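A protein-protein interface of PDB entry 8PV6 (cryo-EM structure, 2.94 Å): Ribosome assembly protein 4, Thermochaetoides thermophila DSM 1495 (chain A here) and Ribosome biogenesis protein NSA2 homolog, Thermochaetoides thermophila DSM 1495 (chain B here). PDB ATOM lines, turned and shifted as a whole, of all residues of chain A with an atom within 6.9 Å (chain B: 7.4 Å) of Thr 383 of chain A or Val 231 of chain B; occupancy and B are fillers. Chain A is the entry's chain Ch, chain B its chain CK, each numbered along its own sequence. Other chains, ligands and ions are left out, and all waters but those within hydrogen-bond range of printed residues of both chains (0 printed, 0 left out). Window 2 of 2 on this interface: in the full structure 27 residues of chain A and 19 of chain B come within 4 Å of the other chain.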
ATOM      1  N   ALA A 319      11.355 -11.390 -27.798  1.00  0.00           N
ATOM      2  CA  ALA A 319      11.821 -12.555 -27.053  1.00  0.00           C
ATOM      3  C   ALA A 319      12.527 -12.175 -25.758  1.00  0.00           C
ATOM      4  O   ALA A 319      12.584 -12.991 -24.832  1.00  0.00           O
ATOM      5  CB  ALA A 319      12.750 -13.398 -27.924  1.00  0.00           C
ATOM      6  N   HIS A 320      13.071 -10.965 -25.674  1.00  0.00           N
ATOM      7  CA  HIS A 320      13.845 -10.572 -24.504  1.00  0.00           C
ATOM      8  C   HIS A 320      12.935 -10.322 -23.308  1.00  0.00           C
ATOM      9  O   HIS A 320      11.771  -9.941 -23.458  1.00  0.00           O
ATOM     10  CB  HIS A 320      14.665  -9.321 -24.806  1.00  0.00           C
ATOM     11  CG  HIS A 320      15.880  -9.583 -25.638  1.00  0.00           C
ATOM     12  ND1 HIS A 320      16.961 -10.300 -25.173  1.00  0.00           N
ATOM     13  CD2 HIS A 320      16.188  -9.217 -26.904  1.00  0.00           C
ATOM     14  CE1 HIS A 320      17.884 -10.361 -26.115  1.00  0.00           C
ATOM     15  NE2 HIS A 320      17.438  -9.717 -27.177  1.00  0.00           N
ATOM     16  N   GLY A 321      13.475 -10.542 -22.114  1.00  0.00           N
ATOM     17  CA  GLY A 321      12.740 -10.395 -20.877  1.00  0.00           C
ATOM     18  C   GLY A 321      12.995  -9.124 -20.100  1.00  0.00           C
ATOM     19  O   GLY A 321      12.438  -8.966 -19.008  1.00  0.00           O
ATOM     20  N   SER A 377      21.250  -9.025 -30.263  1.00  0.00           N
ATOM     21  CA  SER A 377      20.674  -8.098 -29.299  1.00  0.00           C
ATOM     22  C   SER A 377      20.976  -8.576 -27.889  1.00  0.00           C
ATOM     23  O   SER A 377      20.655  -9.713 -27.528  1.00  0.00           O
ATOM     24  CB  SER A 377      19.161  -7.959 -29.492  1.00  0.00           C
ATOM     25  OG  SER A 377      18.532  -9.226 -29.529  1.00  0.00           O
ATOM     26  N   ALA A 378      21.586  -7.705 -27.094  1.00  0.00           N
ATOM     27  CA  ALA A 378      21.966  -8.012 -25.723  1.00  0.00           C
ATOM     28  C   ALA A 378      21.006  -7.325 -24.766  1.00  0.00           C
ATOM     29  O   ALA A 378      20.675  -6.151 -24.953  1.00  0.00           O
ATOM     30  CB  ALA A 378      23.394  -7.550 -25.445  1.00  0.00           C
ATOM     31  N   SER A 379      20.553  -8.042 -23.735  1.00  0.00           N
ATOM     32  CA  SER A 379      19.557  -7.449 -22.855  1.00  0.00           C
ATOM     33  C   SER A 379      19.977  -7.568 -21.399  1.00  0.00           C
ATOM     34  O   SER A 379      21.003  -8.166 -21.067  1.00  0.00           O
ATOM     35  CB  SER A 379      18.182  -8.086 -23.055  1.00  0.00           C
ATOM     36  OG  SER A 379      18.287  -9.494 -23.139  1.00  0.00           O
ATOM     37  N   ASP A 380      19.159  -6.972 -20.532  1.00  0.00           N
ATOM     38  CA  ASP A 380      19.306  -6.982 -19.080  1.00  0.00           C
ATOM     39  C   ASP A 380      18.724  -8.217 -18.442  1.00  0.00           C
ATOM     40  O   ASP A 380      18.806  -8.346 -17.215  1.00  0.00           O
ATOM     41  CB  ASP A 380      18.658  -5.737 -18.476  1.00  0.00           C
ATOM     42  CG  ASP A 380      19.564  -4.528 -18.520  1.00  0.00           C
ATOM     43  OD1 ASP A 380      20.704  -4.661 -19.008  1.00  0.00           O
ATOM     44  OD2 ASP A 380      19.139  -3.447 -18.064  1.00  0.00           O
ATOM     45  N   ASP A 381      18.142  -9.132 -19.214  1.00  0.00           N
ATOM     46  CA  ASP A 381      17.681 -10.410 -18.691  1.00  0.00           C
ATOM     47  C   ASP A 381      18.778 -11.466 -18.679  1.00  0.00           C
ATOM     48  O   ASP A 381      18.469 -12.656 -18.789  1.00  0.00           O
ATOM     49  CB  ASP A 381      16.460 -10.909 -19.479  1.00  0.00           C
ATOM     50  CG  ASP A 381      16.730 -11.084 -20.973  1.00  0.00           C
ATOM     51  OD1 ASP A 381      17.883 -10.950 -21.433  1.00  0.00           O
ATOM     52  OD2 ASP A 381      15.763 -11.378 -21.705  1.00  0.00           O
ATOM     53  N   PHE A 382      20.044 -11.034 -18.618  1.00  0.00           N
ATOM     54  CA  PHE A 382      21.261 -11.847 -18.531  1.00  0.00           C
ATOM     55  C   PHE A 382      21.584 -12.549 -19.842  1.00  0.00           C
ATOM     56  O   PHE A 382      22.505 -13.370 -19.883  1.00  0.00           O
ATOM     57  CB  PHE A 382      21.225 -12.907 -17.413  1.00  0.00           C
ATOM     58  CG  PHE A 382      21.016 -12.367 -16.013  1.00  0.00           C
ATOM     59  CD1 PHE A 382      21.078 -11.012 -15.726  1.00  0.00           C
ATOM     60  CD2 PHE A 382      20.762 -13.246 -14.975  1.00  0.00           C
ATOM     61  CE1 PHE A 382      20.885 -10.549 -14.442  1.00  0.00           C
ATOM     62  CE2 PHE A 382      20.568 -12.788 -13.687  1.00  0.00           C
ATOM     63  CZ  PHE A 382      20.632 -11.438 -13.421  1.00  0.00           C
ATOM     64  N   THR A 383      20.860 -12.260 -20.924  1.00  0.00           N
ATOM     65  CA  THR A 383      20.939 -13.074 -22.129  1.00  0.00           C
ATOM     66  C   THR A 383      21.208 -12.216 -23.356  1.00  0.00           C
ATOM     67  O   THR A 383      21.175 -10.976 -23.320  1.00  0.00           O
ATOM     68  CB  THR A 383      19.652 -13.874 -22.375  1.00  0.00           C
ATOM     69  OG1 THR A 383      18.562 -12.972 -22.596  1.00  0.00           O
ATOM     70  CG2 THR A 383      19.329 -14.770 -21.198  1.00  0.00           C
ATOM     71  N   MET A 384      21.478 -12.918 -24.457  1.00  0.00           N
ATOM     72  CA  MET A 384      21.576 -12.317 -25.776  1.00  0.00           C
ATOM     73  C   MET A 384      20.802 -13.182 -26.758  1.00  0.00           C
ATOM     74  O   MET A 384      20.595 -14.371 -26.525  1.00  0.00           O
ATOM     75  CB  MET A 384      23.031 -12.189 -26.215  1.00  0.00           C
ATOM     76  CG  MET A 384      23.826 -11.215 -25.385  1.00  0.00           C
ATOM     77  SD  MET A 384      25.498 -11.072 -25.989  1.00  0.00           S
ATOM     78  CE  MET A 384      26.121 -12.641 -25.397  1.00  0.00           C
ATOM     79  N   TYR A 385      20.370 -12.575 -27.852  1.00  0.00           N
ATOM     80  CA  TYR A 385      19.669 -13.289 -28.909  1.00  0.00           C
ATOM     81  C   TYR A 385      20.341 -13.024 -30.245  1.00  0.00           C
ATOM     82  O   TYR A 385      20.803 -11.907 -30.507  1.00  0.00           O
ATOM     83  CB  TYR A 385      18.198 -12.886 -28.980  1.00  0.00           C
ATOM     84  CG  TYR A 385      17.263 -13.774 -28.189  1.00  0.00           C
ATOM     85  CD1 TYR A 385      16.792 -14.962 -28.725  1.00  0.00           C
ATOM     86  CD2 TYR A 385      16.833 -13.415 -26.921  1.00  0.00           C
ATOM     87  CE1 TYR A 385      15.932 -15.777 -28.016  1.00  0.00           C
ATOM     88  CE2 TYR A 385      15.973 -14.220 -26.204  1.00  0.00           C
ATOM     89  CZ  TYR A 385      15.525 -15.398 -26.757  1.00  0.00           C
ATOM     90  OH  TYR A 385      14.668 -16.204 -26.045  1.00  0.00           O
ATOM     91  N   ARG A 399      19.979 -18.510 -28.696  1.00  0.00           N
ATOM     92  CA  ARG A 399      19.993 -17.682 -27.499  1.00  0.00           C
ATOM     93  C   ARG A 399      21.341 -17.862 -26.819  1.00  0.00           C
ATOM     94  O   ARG A 399      21.695 -18.973 -26.412  1.00  0.00           O
ATOM     95  CB  ARG A 399      18.854 -18.045 -26.547  1.00  0.00           C
ATOM     96  CG  ARG A 399      18.649 -17.016 -25.447  1.00  0.00           C
ATOM     97  CD  ARG A 399      17.458 -17.351 -24.569  1.00  0.00           C
ATOM     98  NE  ARG A 399      17.020 -16.192 -23.801  1.00  0.00           N
ATOM     99  CZ  ARG A 399      16.043 -16.210 -22.905  1.00  0.00           C
ATOM    100  NH1 ARG A 399      15.379 -17.321 -22.629  1.00  0.00           N
ATOM    101  NH2 ARG A 399      15.723 -15.087 -22.270  1.00  0.00           N
ATOM    102  N   LEU A 400      22.085 -16.771 -26.706  1.00  0.00           N
ATOM    103  CA  LEU A 400      23.416 -16.779 -26.118  1.00  0.00           C
ATOM    104  C   LEU A 400      23.252 -16.651 -24.608  1.00  0.00           C
ATOM    105  O   LEU A 400      22.797 -15.612 -24.106  1.00  0.00           O
ATOM    106  CB  LEU A 400      24.270 -15.654 -26.704  1.00  0.00           C
ATOM    107  CG  LEU A 400      24.914 -15.850 -28.090  1.00  0.00           C
ATOM    108  CD1 LEU A 400      23.915 -15.888 -29.241  1.00  0.00           C
ATOM    109  CD2 LEU A 400      25.927 -14.762 -28.359  1.00  0.00           C
ATOM    110  N   LEU A 401      23.605 -17.725 -23.899  1.00  0.00           N
ATOM    111  CA  LEU A 401      23.383 -17.892 -22.471  1.00  0.00           C
ATOM    112  C   LEU A 401      24.714 -18.095 -21.766  1.00  0.00           C
ATOM    113  O   LEU A 401      25.611 -18.754 -22.298  1.00  0.00           O
ATOM    114  CB  LEU A 401      22.490 -19.105 -22.188  1.00  0.00           C
ATOM    115  CG  LEU A 401      21.106 -19.194 -22.826  1.00  0.00           C
ATOM    116  CD1 LEU A 401      20.522 -20.577 -22.620  1.00  0.00           C
ATOM    117  CD2 LEU A 401      20.203 -18.161 -22.218  1.00  0.00           C
ATOM    118  N   GLY A 402      24.822 -17.575 -20.549  1.00  0.00           N
ATOM    119  CA  GLY A 402      26.030 -17.766 -19.772  1.00  0.00           C
ATOM    120  C   GLY A 402      26.417 -16.574 -18.926  1.00  0.00           C
ATOM    121  O   GLY A 402      27.092 -16.730 -17.905  1.00  0.00           O
ATOM    122  N   HIS A 403      26.003 -15.379 -19.336  1.00  0.00           N
ATOM    123  CA  HIS A 403      26.208 -14.206 -18.501  1.00  0.00           C
ATOM    124  C   HIS A 403      25.288 -14.263 -17.291  1.00  0.00           C
ATOM    125  O   HIS A 403      24.087 -14.515 -17.417  1.00  0.00           O
ATOM    126  CB  HIS A 403      25.949 -12.930 -19.297  1.00  0.00           C
ATOM    127  CG  HIS A 403      27.140 -12.438 -20.059  1.00  0.00           C
ATOM    128  ND1 HIS A 403      28.182 -11.770 -19.456  1.00  0.00           N
ATOM    129  CD2 HIS A 403      27.447 -12.507 -21.375  1.00  0.00           C
ATOM    130  CE1 HIS A 403      29.085 -11.455 -20.368  1.00  0.00           C
ATOM    131  NE2 HIS A 403      28.662 -11.891 -21.540  1.00  0.00           N
ATOM    132  N   ASN A 405      24.979 -11.657 -15.144  1.00  0.00           N
ATOM    133  CA  ASN A 405      24.504 -10.315 -14.835  1.00  0.00           C
ATOM    134  C   ASN A 405      24.097  -9.665 -16.152  1.00  0.00           C
ATOM    135  O   ASN A 405      24.034 -10.323 -17.193  1.00  0.00           O
ATOM    136  CB  ASN A 405      25.562  -9.501 -14.088  1.00  0.00           C
ATOM    137  CG  ASN A 405      24.951  -8.480 -13.148  1.00  0.00           C
ATOM    138  OD1 ASN A 405      23.810  -8.059 -13.330  1.00  0.00           O
ATOM    139  ND2 ASN A 405      25.707  -8.081 -12.133  1.00  0.00           N
ATOM    140  N   LYS A 406      23.789  -8.370 -16.093  1.00  0.00           N
ATOM    141  CA  LYS A 406      23.330  -7.660 -17.280  1.00  0.00           C
ATOM    142  C   LYS A 406      24.445  -7.556 -18.312  1.00  0.00           C
ATOM    143  O   LYS A 406      25.619  -7.401 -17.970  1.00  0.00           O
ATOM    144  CB  LYS A 406      22.831  -6.265 -16.905  1.00  0.00           C
ATOM    145  CG  LYS A 406      21.813  -6.254 -15.782  1.00  0.00           C
ATOM    146  CD  LYS A 406      21.418  -4.838 -15.408  1.00  0.00           C
ATOM    147  CE  LYS A 406      22.574  -4.085 -14.782  1.00  0.00           C
ATOM    148  NZ  LYS A 406      22.968  -4.683 -13.477  1.00  0.00           N
ATOM    149  N   VAL A 407      24.072  -7.663 -19.583  1.00  0.00           N
ATOM    150  CA  VAL A 407      25.020  -7.557 -20.684  1.00  0.00           C
ATOM    151  C   VAL A 407      24.916  -6.148 -21.244  1.00  0.00           C
ATOM    152  O   VAL A 407      23.841  -5.722 -21.682  1.00  0.00           O
ATOM    153  CB  VAL A 407      24.745  -8.605 -21.772  1.00  0.00           C
ATOM    154  CG1 VAL A 407      25.780  -8.490 -22.871  1.00  0.00           C
ATOM    155  CG2 VAL A 407      24.733  -9.998 -21.178  1.00  0.00           C
ATOM    156  N   VAL B 225       6.233 -16.046 -11.809  1.00  0.00           N
ATOM    157  CA  VAL B 225       6.735 -14.997 -12.688  1.00  0.00           C
ATOM    158  C   VAL B 225       7.138 -15.595 -14.029  1.00  0.00           C
ATOM    159  O   VAL B 225       8.031 -15.082 -14.713  1.00  0.00           O
ATOM    160  CB  VAL B 225       7.893 -14.230 -12.022  1.00  0.00           C
ATOM    161  CG1 VAL B 225       7.401 -13.546 -10.765  1.00  0.00           C
ATOM    162  CG2 VAL B 225       9.021 -15.173 -11.658  1.00  0.00           C
ATOM    163  N   LEU B 228       7.016 -13.268 -17.141  1.00  0.00           N
ATOM    164  CA  LEU B 228       7.938 -12.143 -17.204  1.00  0.00           C
ATOM    165  C   LEU B 228       9.274 -12.516 -17.828  1.00  0.00           C
ATOM    166  O   LEU B 228      10.085 -11.628 -18.111  1.00  0.00           O
ATOM    167  CB  LEU B 228       8.153 -11.564 -15.805  1.00  0.00           C
ATOM    168  CG  LEU B 228       6.976 -10.763 -15.252  1.00  0.00           C
ATOM    169  CD1 LEU B 228       7.367 -10.078 -13.963  1.00  0.00           C
ATOM    170  CD2 LEU B 228       6.486  -9.744 -16.271  1.00  0.00           C
ATOM    171  N   GLY B 229       9.518 -13.802 -18.057  1.00  0.00           N
ATOM    172  CA  GLY B 229      10.750 -14.241 -18.692  1.00  0.00           C
ATOM    173  C   GLY B 229      12.001 -14.033 -17.865  1.00  0.00           C
ATOM    174  O   GLY B 229      13.061 -13.717 -18.420  1.00  0.00           O
ATOM    175  N   ILE B 230      11.906 -14.205 -16.554  1.00  0.00           N
ATOM    176  CA  ILE B 230      13.075 -14.171 -15.684  1.00  0.00           C
ATOM    177  C   ILE B 230      13.782 -15.510 -15.790  1.00  0.00           C
ATOM    178  O   ILE B 230      13.176 -16.567 -15.581  1.00  0.00           O
ATOM    179  CB  ILE B 230      12.679 -13.858 -14.230  1.00  0.00           C
ATOM    180  CG1 ILE B 230      11.774 -12.627 -14.177  1.00  0.00           C
ATOM    181  CG2 ILE B 230      13.919 -13.645 -13.379  1.00  0.00           C
ATOM    182  CD1 ILE B 230      11.323 -12.264 -12.782  1.00  0.00           C
ATOM    183  N   VAL B 231      15.074 -15.473 -16.117  1.00  0.00           N
ATOM    184  CA  VAL B 231      15.823 -16.675 -16.451  1.00  0.00           C
ATOM    185  C   VAL B 231      17.106 -16.712 -15.627  1.00  0.00           C
ATOM    186  O   VAL B 231      17.676 -15.679 -15.268  1.00  0.00           O
ATOM    187  CB  VAL B 231      16.113 -16.743 -17.977  1.00  0.00           C
ATOM    188  CG1 VAL B 231      17.070 -15.648 -18.410  1.00  0.00           C
ATOM    189  CG2 VAL B 231      16.599 -18.121 -18.408  1.00  0.00           C
ATOM    190  N   THR B 232      17.525 -17.927 -15.284  1.00  0.00           N
ATOM    191  CA  THR B 232      18.780 -18.163 -14.591  1.00  0.00           C
ATOM    192  C   THR B 232      19.925 -18.031 -15.602  1.00  0.00           C
ATOM    193  O   THR B 232      19.706 -17.946 -16.814  1.00  0.00           O
ATOM    194  CB  THR B 232      18.729 -19.535 -13.912  1.00  0.00           C
ATOM    195  OG1 THR B 232      17.436 -19.711 -13.326  1.00  0.00           O
ATOM    196  CG2 THR B 232      19.737 -19.644 -12.772  1.00  0.00           C
ATOM    197  N   ALA B 233      21.165 -18.008 -15.111  1.00  0.00           N
ATOM    198  CA  ALA B 233      22.346 -17.751 -15.928  1.00  0.00           C
ATOM    199  C   ALA B 233      22.632 -18.832 -16.965  1.00  0.00           C
ATOM    200  O   ALA B 233      23.443 -18.594 -17.864  1.00  0.00           O
ATOM    201  CB  ALA B 233      23.572 -17.582 -15.029  1.00  0.00           C
ATOM    202  N   SER B 234      21.999 -20.003 -16.876  1.00  0.00           N
ATOM    203  CA  SER B 234      22.230 -21.067 -17.842  1.00  0.00           C
ATOM    204  C   SER B 234      21.019 -21.406 -18.693  1.00  0.00           C
ATOM    205  O   SER B 234      21.167 -22.151 -19.669  1.00  0.00           O
ATOM    206  CB  SER B 234      22.703 -22.344 -17.134  1.00  0.00           C
ATOM    207  OG  SER B 234      21.706 -22.844 -16.263  1.00  0.00           O
ATOM    208  N   GLY B 235      19.836 -20.894 -18.367  1.00  0.00           N
ATOM    209  CA  GLY B 235      18.632 -21.147 -19.133  1.00  0.00           C
ATOM    210  C   GLY B 235      17.456 -21.634 -18.316  1.00  0.00           C
ATOM    211  O   GLY B 235      16.364 -21.816 -18.873  1.00  0.00           O
ATOM    212  N   LYS B 236      17.639 -21.867 -17.018  1.00  0.00           N
ATOM    213  CA  LYS B 236      16.535 -22.301 -16.176  1.00  0.00           C
ATOM    214  C   LYS B 236      15.537 -21.168 -15.983  1.00  0.00           C
ATOM    215  O   LYS B 236      15.915 -20.019 -15.745  1.00  0.00           O
ATOM    216  CB  LYS B 236      17.060 -22.774 -14.821  1.00  0.00           C
ATOM    217  CG  LYS B 236      18.078 -23.895 -14.902  1.00  0.00           C
ATOM    218  CD  LYS B 236      18.596 -24.263 -13.525  1.00  0.00           C
ATOM    219  CE  LYS B 236      19.589 -25.411 -13.597  1.00  0.00           C
ATOM    220  NZ  LYS B 236      20.208 -25.695 -12.273  1.00  0.00           N
ATOM    221  N   ILE B 237      14.254 -21.496 -16.078  1.00  0.00           N
ATOM    222  CA  ILE B 237      13.205 -20.502 -15.889  1.00  0.00           C
ATOM    223  C   ILE B 237      12.990 -20.281 -14.401  1.00  0.00           C
ATOM    224  O   ILE B 237      12.705 -21.224 -13.656  1.00  0.00           O
ATOM    225  CB  ILE B 237      11.898 -20.938 -16.566  1.00  0.00           C
ATOM    226  CG1 ILE B 237      12.071 -21.058 -18.075  1.00  0.00           C
ATOM    227  CG2 ILE B 237      10.782 -19.959 -16.245  1.00  0.00           C
ATOM    228  CD1 ILE B 237      10.895 -21.726 -18.749  1.00  0.00           C
ATOM    229  N   ALA B 238      13.119 -19.034 -13.966  1.00  0.00           N
ATOM    230  CA  ALA B 238      12.706 -18.642 -12.627  1.00  0.00           C
ATOM    231  C   ALA B 238      11.193 -18.470 -12.633  1.00  0.00           C
ATOM    232  O   ALA B 238      10.680 -17.502 -13.201  1.00  0.00           O
ATOM    233  CB  ALA B 238      13.397 -17.351 -12.198  1.00  0.00           C
ATOM    234  N   TRP B 239      10.480 -19.419 -12.031  1.00  0.00           N
ATOM    235  CA  TRP B 239       9.025 -19.395 -12.028  1.00  0.00           C
ATOM    236  C   TRP B 239       8.427 -19.141 -10.652  1.00  0.00           C
ATOM    237  O   TRP B 239       7.216 -19.298 -10.481  1.00  0.00           O
ATOM    238  CB  TRP B 239       8.473 -20.700 -12.616  1.00  0.00           C
ATOM    239  CG  TRP B 239       8.613 -21.906 -11.749  1.00  0.00           C
ATOM    240  CD1 TRP B 239       9.743 -22.634 -11.537  1.00  0.00           C
ATOM    241  CD2 TRP B 239       7.576 -22.546 -10.999  1.00  0.00           C
ATOM    242  NE1 TRP B 239       9.479 -23.684 -10.692  1.00  0.00           N
ATOM    243  CE2 TRP B 239       8.154 -23.652 -10.348  1.00  0.00           C
ATOM    244  CE3 TRP B 239       6.215 -22.289 -10.810  1.00  0.00           C
ATOM    245  CZ2 TRP B 239       7.420 -24.496  -9.523  1.00  0.00           C
ATOM    246  CZ3 TRP B 239       5.490 -23.128  -9.990  1.00  0.00           C
ATOM    247  CH2 TRP B 239       6.092 -24.218  -9.357  1.00  0.00           C
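The backbone NH of Gly 402 of chain A lies within hydrogen-bond range of the backbone carbonyl oxygen of Ala 233 of chain B, 3.2 Å away.
The side-chain hydroxyl (OG) of Ser 379 of chain A lies within hydrogen-bond range of the backbone carbonyl oxygen (O) of Thr 383 of chain A, at 3.3 Å. The side-chain carboxylate (OD1) of Asp 381 of chain A sits at hydrogen-bond distance from the side-chain hydroxyl (OG1) of Thr 383 of chain A. N of Gly 321 of chain A is in hydrogen-bond range of OD2 of Asp 381 of chain A. The side-chain carboxylate (OD2) of Asp 381 of chain A is in salt-bridge range of the guanidinium group (NH2) of Arg 399 of chain A (3.8 Å). OD2 of Asp 381 of chain A lies close to OG of Ser 379 of chain A (3.5 Å).
Among the printed residues, pairs that only touch across the chains: Asp 381 of chain A with Val 231 of chain B (3.3 Å), Leu 401 of chain A with Ser 234 of chain B (3.4 Å), Gly 321 of chain A with Leu 228 of chain B (3.7 Å), Thr 383 of chain A with Val 231 of chain B (3.7 Å), His 403 of chain A with Ala 233 of chain B (3.9 Å) and Phe 382 of chain A with Val 231 of chain B (3.9 Å).
Thr 383 of chain A touches just one residue of chain B: Val 231 (3.7 Å). Of chain A, only Asp 381 (3.3 Å), Phe 382 (3.9 Å) and Thr 383 (3.7 Å) come within 4 Å of Val 231 of chain B. Of the printed residues of chain B, His 403 of chain A touches Ala 233 (3.9 Å). Of the printed residues of chain B, Leu 401 of chain A touches Ser 234 (3.4 Å). Printed residues of chain B within 4 Å of Phe 382 of chain A: Val 231. Printed residues of chain B within 4 Å of Asp 381 of chain A: Val 231 (3.3 Å). Asp 380 of chain A touches none of the printed residues of chain B. The nearest residue of chain B that does not touch Thr 383 of chain A is Thr 232 of chain B (5.4 Å). The nearest residue of chain A that does not touch Val 231 of chain B is Arg 399 of chain A (4.1 Å). The nearest printed residue of chain B that does not touch Gly 321 of chain A is Gly 229 of chain B (4.1 Å).
Hydrophobic or aromatic side chains of chain A within 4 Å of the printed part of chain B: Phe 382 and Leu 401. Along chain A the printed residues that touch a printed residue of chain B span positions 321 to 403. Of the 13 printed residues of chain B, 4 touch a printed residue of chain A. Hydrophobic or aromatic side chains of chain B within 4 Å of the printed part of chain A: Val 231 and Ala 233. Among the printed residues, no Asp or Glu carboxylate lies within 4 Å of a Lys or Arg side-chain nitrogen of the other chain.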
